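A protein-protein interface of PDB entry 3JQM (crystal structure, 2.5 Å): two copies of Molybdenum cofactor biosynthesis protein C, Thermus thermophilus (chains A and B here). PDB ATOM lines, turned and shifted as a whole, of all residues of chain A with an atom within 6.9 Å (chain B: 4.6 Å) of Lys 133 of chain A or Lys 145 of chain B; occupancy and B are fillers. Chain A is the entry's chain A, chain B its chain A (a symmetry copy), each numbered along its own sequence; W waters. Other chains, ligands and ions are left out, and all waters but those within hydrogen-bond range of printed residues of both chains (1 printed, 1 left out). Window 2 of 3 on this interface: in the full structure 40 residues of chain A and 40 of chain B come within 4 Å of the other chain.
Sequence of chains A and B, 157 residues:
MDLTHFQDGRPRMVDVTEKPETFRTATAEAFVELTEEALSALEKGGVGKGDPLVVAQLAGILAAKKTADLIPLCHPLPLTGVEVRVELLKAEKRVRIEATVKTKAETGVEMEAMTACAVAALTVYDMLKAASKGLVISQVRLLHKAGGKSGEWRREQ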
ATOM      1  N   THR A  35     -17.047 -13.746 -29.077  1.00  0.00           N
ATOM      2  CA  THR A  35     -17.114 -12.825 -30.211  1.00  0.00           C
ATOM      3  C   THR A  35     -16.526 -13.657 -31.344  1.00  0.00           C
ATOM      4  O   THR A  35     -15.875 -14.677 -31.096  1.00  0.00           O
ATOM      5  CB  THR A  35     -16.232 -11.557 -30.018  1.00  0.00           C
ATOM      6  OG1 THR A  35     -14.872 -11.943 -29.788  1.00  0.00           O
ATOM      7  CG2 THR A  35     -16.723 -10.724 -28.850  1.00  0.00           C
ATOM      8  N   GLU A  37     -13.976 -13.111 -33.281  1.00  0.00           N
ATOM      9  CA  GLU A  37     -12.516 -13.177 -33.171  1.00  0.00           C
ATOM     10  C   GLU A  37     -12.082 -14.204 -32.129  1.00  0.00           C
ATOM     11  O   GLU A  37     -11.193 -15.024 -32.378  1.00  0.00           O
ATOM     12  CB  GLU A  37     -11.942 -11.807 -32.792  1.00  0.00           C
ATOM     13  CG  GLU A  37     -12.449 -10.646 -33.652  1.00  0.00           C
ATOM     14  CD  GLU A  37     -13.718  -9.999 -33.093  1.00  0.00           C
ATOM     15  OE1 GLU A  37     -13.614  -9.288 -32.063  1.00  0.00           O
ATOM     16  OE2 GLU A  37     -14.813 -10.201 -33.672  1.00  0.00           O
ATOM     17  N   TYR A 125     -12.021 -16.625 -20.087  1.00  0.00           N
ATOM     18  CA  TYR A 125     -11.794 -15.218 -20.398  1.00  0.00           C
ATOM     19  C   TYR A 125     -10.309 -14.868 -20.415  1.00  0.00           C
ATOM     20  O   TYR A 125      -9.835 -14.184 -21.322  1.00  0.00           O
ATOM     21  CB  TYR A 125     -12.504 -14.321 -19.379  1.00  0.00           C
ATOM     22  CG  TYR A 125     -12.358 -12.852 -19.682  1.00  0.00           C
ATOM     23  CD1 TYR A 125     -13.129 -12.250 -20.669  1.00  0.00           C
ATOM     24  CD2 TYR A 125     -11.414 -12.075 -19.017  1.00  0.00           C
ATOM     25  CE1 TYR A 125     -12.963 -10.905 -20.990  1.00  0.00           C
ATOM     26  CE2 TYR A 125     -11.235 -10.736 -19.326  1.00  0.00           C
ATOM     27  CZ  TYR A 125     -12.011 -10.153 -20.313  1.00  0.00           C
ATOM     28  OH  TYR A 125     -11.839  -8.822 -20.625  1.00  0.00           O
ATOM     29  N   LEU A 128      -8.504 -16.126 -23.483  1.00  0.00           N
ATOM     30  CA  LEU A 128      -8.905 -15.606 -24.781  1.00  0.00           C
ATOM     31  C   LEU A 128      -9.005 -14.089 -24.886  1.00  0.00           C
ATOM     32  O   LEU A 128      -9.212 -13.567 -25.978  1.00  0.00           O
ATOM     33  CB  LEU A 128     -10.254 -16.212 -25.191  1.00  0.00           C
ATOM     34  CG  LEU A 128     -10.384 -17.725 -25.403  1.00  0.00           C
ATOM     35  CD1 LEU A 128     -11.837 -18.061 -25.668  1.00  0.00           C
ATOM     36  CD2 LEU A 128      -9.501 -18.184 -26.574  1.00  0.00           C
ATOM     37  N   LYS A 129      -8.860 -13.378 -23.770  1.00  0.00           N
ATOM     38  CA  LYS A 129      -8.965 -11.922 -23.793  1.00  0.00           C
ATOM     39  C   LYS A 129      -7.974 -11.254 -24.746  1.00  0.00           C
ATOM     40  O   LYS A 129      -8.203 -10.121 -25.191  1.00  0.00           O
ATOM     41  CB  LYS A 129      -8.813 -11.338 -22.384  1.00  0.00           C
ATOM     42  CG  LYS A 129      -7.412 -11.315 -21.799  1.00  0.00           C
ATOM     43  CD  LYS A 129      -7.452 -10.582 -20.446  1.00  0.00           C
ATOM     44  CE  LYS A 129      -6.083 -10.376 -19.827  1.00  0.00           C
ATOM     45  NZ  LYS A 129      -5.428 -11.669 -19.551  1.00  0.00           N
ATOM     46  N   ALA A 130      -6.881 -11.950 -25.063  1.00  0.00           N
ATOM     47  CA  ALA A 130      -5.879 -11.421 -25.984  1.00  0.00           C
ATOM     48  C   ALA A 130      -6.532 -11.177 -27.343  1.00  0.00           C
ATOM     49  O   ALA A 130      -6.126 -10.273 -28.077  1.00  0.00           O
ATOM     50  CB  ALA A 130      -4.734 -12.397 -26.132  1.00  0.00           C
ATOM     51  N   ALA A 131      -7.548 -11.982 -27.667  1.00  0.00           N
ATOM     52  CA  ALA A 131      -8.266 -11.865 -28.937  1.00  0.00           C
ATOM     53  C   ALA A 131      -9.446 -10.888 -28.847  1.00  0.00           C
ATOM     54  O   ALA A 131      -9.642 -10.056 -29.738  1.00  0.00           O
ATOM     55  CB  ALA A 131      -8.759 -13.248 -29.398  1.00  0.00           C
ATOM     56  N   SER A 132     -10.239 -10.996 -27.783  1.00  0.00           N
ATOM     57  CA  SER A 132     -11.383 -10.108 -27.589  1.00  0.00           C
ATOM     58  C   SER A 132     -11.542  -9.767 -26.118  1.00  0.00           C
ATOM     59  O   SER A 132     -11.914 -10.628 -25.321  1.00  0.00           O
ATOM     60  CB  SER A 132     -12.682 -10.764 -28.071  1.00  0.00           C
ATOM     61  OG  SER A 132     -12.618 -11.127 -29.436  1.00  0.00           O
ATOM     62  N   LYS A 133     -11.273  -8.522 -25.744  1.00  0.00           N
ATOM     63  CA  LYS A 133     -11.439  -8.144 -24.349  1.00  0.00           C
ATOM     64  C   LYS A 133     -12.913  -8.039 -23.975  1.00  0.00           C
ATOM     65  O   LYS A 133     -13.264  -8.064 -22.798  1.00  0.00           O
ATOM     66  CB  LYS A 133     -10.731  -6.819 -24.067  1.00  0.00           C
ATOM     67  CG  LYS A 133      -9.243  -6.981 -23.852  1.00  0.00           C
ATOM     68  CD  LYS A 133      -8.517  -5.656 -23.877  1.00  0.00           C
ATOM     69  CE  LYS A 133      -7.050  -5.876 -23.569  1.00  0.00           C
ATOM     70  NZ  LYS A 133      -6.235  -4.678 -23.874  1.00  0.00           N
ATOM     71  N   GLY A 134     -13.773  -7.950 -24.986  1.00  0.00           N
ATOM     72  CA  GLY A 134     -15.203  -7.811 -24.753  1.00  0.00           C
ATOM     73  C   GLY A 134     -15.987  -9.062 -24.421  1.00  0.00           C
ATOM     74  O   GLY A 134     -17.184  -8.974 -24.141  1.00  0.00           O
ATOM     75  N   LEU A 135     -15.334 -10.221 -24.453  1.00  0.00           N
ATOM     76  CA  LEU A 135     -16.012 -11.476 -24.136  1.00  0.00           C
ATOM     77  C   LEU A 135     -16.771 -11.368 -22.834  1.00  0.00           C
ATOM     78  O   LEU A 135     -16.308 -10.731 -21.897  1.00  0.00           O
ATOM     79  CB  LEU A 135     -14.995 -12.599 -23.958  1.00  0.00           C
ATOM     80  CG  LEU A 135     -14.127 -12.813 -25.191  1.00  0.00           C
ATOM     81  CD1 LEU A 135     -13.158 -13.967 -24.956  1.00  0.00           C
ATOM     82  CD2 LEU A 135     -15.037 -13.082 -26.371  1.00  0.00           C
ATOM     83  N   VAL A 136     -17.938 -11.988 -22.761  1.00  0.00           N
ATOM     84  CA  VAL A 136     -18.720 -11.895 -21.542  1.00  0.00           C
ATOM     85  C   VAL A 136     -19.049 -13.215 -20.852  1.00  0.00           C
ATOM     86  O   VAL A 136     -19.220 -14.257 -21.505  1.00  0.00           O
ATOM     87  CB  VAL A 136     -20.038 -11.166 -21.882  1.00  0.00           C
ATOM     88  CG1 VAL A 136     -20.878 -10.988 -20.653  1.00  0.00           C
ATOM     89  CG2 VAL A 136     -19.732  -9.822 -22.490  1.00  0.00           C
ATOM     90  N   THR B  25      -4.441  -0.085 -15.547  1.00  0.00           N
ATOM     91  CA  THR B  25      -5.737   0.107 -14.920  1.00  0.00           C
ATOM     92  C   THR B  25      -6.832  -0.654 -15.656  1.00  0.00           C
ATOM     93  O   THR B  25      -6.825  -0.736 -16.878  1.00  0.00           O
ATOM     94  CB  THR B  25      -6.101   1.610 -14.837  1.00  0.00           C
ATOM     95  OG1 THR B  25      -7.266   1.764 -14.024  1.00  0.00           O
ATOM     96  CG2 THR B  25      -6.388   2.182 -16.218  1.00  0.00           C
ATOM     97  N   ALA B  26      -7.763  -1.223 -14.903  1.00  0.00           N
ATOM     98  CA  ALA B  26      -8.871  -1.967 -15.494  1.00  0.00           C
ATOM     99  C   ALA B  26     -10.142  -1.788 -14.676  1.00  0.00           C
ATOM    100  O   ALA B  26     -10.098  -1.657 -13.447  1.00  0.00           O
ATOM    101  CB  ALA B  26      -8.521  -3.455 -15.601  1.00  0.00           C
ATOM    102  N   GLU B 110      -6.816  -6.694 -15.891  1.00  0.00           N
ATOM    103  CA  GLU B 110      -8.169  -7.049 -16.273  1.00  0.00           C
ATOM    104  C   GLU B 110      -8.685  -8.244 -15.477  1.00  0.00           C
ATOM    105  O   GLU B 110      -9.866  -8.295 -15.150  1.00  0.00           O
ATOM    106  CB  GLU B 110      -8.236  -7.360 -17.763  1.00  0.00           C
ATOM    107  CG  GLU B 110      -7.678  -6.261 -18.631  1.00  0.00           C
ATOM    108  CD  GLU B 110      -6.218  -6.469 -18.987  1.00  0.00           C
ATOM    109  OE1 GLU B 110      -5.421  -6.798 -18.071  1.00  0.00           O
ATOM    110  OE2 GLU B 110      -5.872  -6.290 -20.183  1.00  0.00           O
ATOM    111  N   LEU B 142     -15.726  -6.628 -19.007  1.00  0.00           N
ATOM    112  CA  LEU B 142     -14.755  -5.563 -18.845  1.00  0.00           C
ATOM    113  C   LEU B 142     -15.354  -4.279 -19.434  1.00  0.00           C
ATOM    114  O   LEU B 142     -15.940  -4.302 -20.528  1.00  0.00           O
ATOM    115  CB  LEU B 142     -13.470  -5.930 -19.571  1.00  0.00           C
ATOM    116  CG  LEU B 142     -12.264  -5.049 -19.284  1.00  0.00           C
ATOM    117  CD1 LEU B 142     -11.845  -5.208 -17.835  1.00  0.00           C
ATOM    118  CD2 LEU B 142     -11.138  -5.440 -20.211  1.00  0.00           C
ATOM    119  N   HIS B 144     -13.475  -1.030 -19.085  1.00  0.00           N
ATOM    120  CA  HIS B 144     -12.353  -0.208 -19.510  1.00  0.00           C
ATOM    121  C   HIS B 144     -11.024  -0.765 -19.019  1.00  0.00           C
ATOM    122  O   HIS B 144     -10.968  -1.502 -18.038  1.00  0.00           O
ATOM    123  CB  HIS B 144     -12.537   1.231 -19.006  1.00  0.00           C
ATOM    124  CG  HIS B 144     -11.319   2.091 -19.152  1.00  0.00           C
ATOM    125  ND1 HIS B 144     -10.441   2.324 -18.114  1.00  0.00           N
ATOM    126  CD2 HIS B 144     -10.823   2.758 -20.222  1.00  0.00           C
ATOM    127  CE1 HIS B 144      -9.458   3.099 -18.539  1.00  0.00           C
ATOM    128  NE2 HIS B 144      -9.666   3.376 -19.813  1.00  0.00           N
ATOM    129  N   LYS B 145      -9.960  -0.395 -19.720  1.00  0.00           N
ATOM    130  CA  LYS B 145      -8.610  -0.825 -19.401  1.00  0.00           C
ATOM    131  C   LYS B 145      -7.655   0.170 -20.043  1.00  0.00           C
ATOM    132  O   LYS B 145      -7.977   0.752 -21.079  1.00  0.00           O
ATOM    133  CB  LYS B 145      -8.359  -2.214 -19.969  1.00  0.00           C
ATOM    134  CG  LYS B 145      -6.933  -2.690 -19.828  1.00  0.00           C
ATOM    135  CD  LYS B 145      -6.466  -3.290 -21.136  1.00  0.00           C
ATOM    136  CE  LYS B 145      -6.174  -2.215 -22.187  1.00  0.00           C
ATOM    137  NZ  LYS B 145      -4.871  -1.501 -21.968  1.00  0.00           N
ATOM    138  N   ALA B 146      -6.485   0.358 -19.434  1.00  0.00           N
ATOM    139  CA  ALA B 146      -5.489   1.298 -19.943  1.00  0.00           C
ATOM    140  C   ALA B 146      -4.068   0.957 -19.490  1.00  0.00           C
ATOM    141  O   ALA B 146      -3.870   0.293 -18.479  1.00  0.00           O
ATOM    142  CB  ALA B 146      -5.843   2.718 -19.506  1.00  0.00           C
ATOM    143  N   GLY B 147      -3.084   1.426 -20.247  1.00  0.00           N
ATOM    144  CA  GLY B 147      -1.703   1.162 -19.901  1.00  0.00           C
ATOM    145  C   GLY B 147      -0.974   0.320 -20.931  1.00  0.00           C
ATOM    146  O   GLY B 147      -1.527  -0.635 -21.490  1.00  0.00           O
ATOM    147  N   SER B 150      -1.535  -1.491 -26.043  1.00  0.00           N
ATOM    148  CA  SER B 150      -2.847  -1.273 -26.648  1.00  0.00           C
ATOM    149  C   SER B 150      -3.455   0.027 -26.133  1.00  0.00           C
ATOM    150  O   SER B 150      -4.355   0.587 -26.759  1.00  0.00           O
ATOM    151  CB  SER B 150      -3.799  -2.429 -26.335  1.00  0.00           C
ATOM    152  OG  SER B 150      -3.426  -3.606 -27.031  1.00  0.00           O
ATOM    153  N   GLY B 151      -2.972   0.510 -24.995  1.00  0.00           N
ATOM    154  CA  GLY B 151      -3.516   1.743 -24.460  1.00  0.00           C
ATOM    155  C   GLY B 151      -4.994   1.655 -24.116  1.00  0.00           C
ATOM    156  O   GLY B 151      -5.584   0.575 -24.108  1.00  0.00           O
ATOM    157  N   GLU B 152      -5.591   2.811 -23.842  1.00  0.00           N
ATOM    158  CA  GLU B 152      -6.993   2.910 -23.464  1.00  0.00           C
ATOM    159  C   GLU B 152      -7.928   2.042 -24.307  1.00  0.00           C
ATOM    160  O   GLU B 152      -7.926   2.119 -25.540  1.00  0.00           O
ATOM    161  CB  GLU B 152      -7.436   4.380 -23.531  1.00  0.00           C
ATOM    162  CG  GLU B 152      -8.316   4.839 -22.365  1.00  0.00           C
ATOM    163  CD  GLU B 152      -7.724   6.022 -21.596  1.00  0.00           C
ATOM    164  OE1 GLU B 152      -7.386   7.040 -22.242  1.00  0.00           O
ATOM    165  OE2 GLU B 152      -7.601   5.944 -20.349  1.00  0.00           O
ATOM    166  N   TRP B 153      -8.709   1.202 -23.627  1.00  0.00           N
ATOM    167  CA  TRP B 153      -9.691   0.332 -24.276  1.00  0.00           C
ATOM    168  C   TRP B 153     -11.027   0.606 -23.601  1.00  0.00           C
ATOM    169  O   TRP B 153     -11.090   0.778 -22.388  1.00  0.00           O
ATOM    170  CB  TRP B 153      -9.351  -1.148 -24.104  1.00  0.00           C
ATOM    171  CG  TRP B 153     -10.343  -2.039 -24.794  1.00  0.00           C
ATOM    172  CD1 TRP B 153     -10.366  -2.365 -26.118  1.00  0.00           C
ATOM    173  CD2 TRP B 153     -11.519  -2.625 -24.218  1.00  0.00           C
ATOM    174  NE1 TRP B 153     -11.480  -3.112 -26.406  1.00  0.00           N
ATOM    175  CE2 TRP B 153     -12.206  -3.289 -25.258  1.00  0.00           C
ATOM    176  CE3 TRP B 153     -12.058  -2.654 -22.923  1.00  0.00           C
ATOM    177  CZ2 TRP B 153     -13.412  -3.971 -25.047  1.00  0.00           C
ATOM    178  CZ3 TRP B 153     -13.259  -3.331 -22.713  1.00  0.00           C
ATOM    179  CH2 TRP B 153     -13.921  -3.984 -23.774  1.00  0.00           C
HETATM  180  O   HOH W   1      -4.100  -6.126 -24.994  1.00  0.00           O
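The side-chain hydroxyl (OH) of Tyr 125 of chain A sits at hydrogen-bond distance from the backbone carbonyl oxygen (O) of Lys 133 of chain A (2.7 Å).
NZ of Lys 145 of chain B lies within hydrogen-bond range of O of Gly 147 of chain B (3.5 Å).
The backbone carbonyl oxygen (O) of Gly 151 of chain B lies within hydrogen-bond range of the side-chain amino group (NZ) of Lys 145 of chain B (3.1 Å).
O of Lys 145 of chain B sits at hydrogen-bond distance from N of Trp 153 of chain B, 2.7 Å away.
Among the printed residues, pairs that only touch across the chains: Tyr 125 of chain A with Leu 142 of chain B, Lys 129 of chain A with Glu 110 of chain B, Lys 133 of chain A with Glu 110 of chain B, Lys 133 of chain A with Leu 142 of chain B, Lys 133 of chain A with Lys 145 of chain B and Gly 134 of chain A with Trp 153 of chain B.
Of the printed residues of chain B, Lys 133 of chain A touches Glu 110, Leu 142 and Lys 145.
Printed residues of chain A within 4 Å of Trp 153 of chain B: Gly 134 (3.996 Å).
Printed residues of chain B within 4 Å of Tyr 125 of chain A: Leu 142.
Printed residues of chain A within 4 Å of Glu 110 of chain B: Lys 129 (3.999 Å) and Lys 133 (3.6 Å).
Of the printed residues of chain B, Lys 129 of chain A touches Glu 110.
The nearest printed residue of chain A that does not touch Lys 145 of chain B is Lys 129 of chain A (7.2 Å).
Along chain A the printed residues that touch a printed residue of chain B span positions 125 to 134.
Printed residues of chain B that touch a printed residue of chain A: Glu 110, Leu 142, Lys 145 and Trp 153.
Hydrophobic or aromatic side chains of chain B within 4 Å of the printed part of chain A: Leu 142 and Trp 153.
Among the printed residues, 6 pairs touch across the chains.
Among the printed residues, no Asp or Glu carboxylate lies within 4 Å of a Lys or Arg side-chain nitrogen of the other chain.
No position is printed for both chains.
Water W1 bridges the side-chain amino group (NZ) of Lys 133 of chain A and the side-chain hydroxyl (OG) of Ser 150 of chain B.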
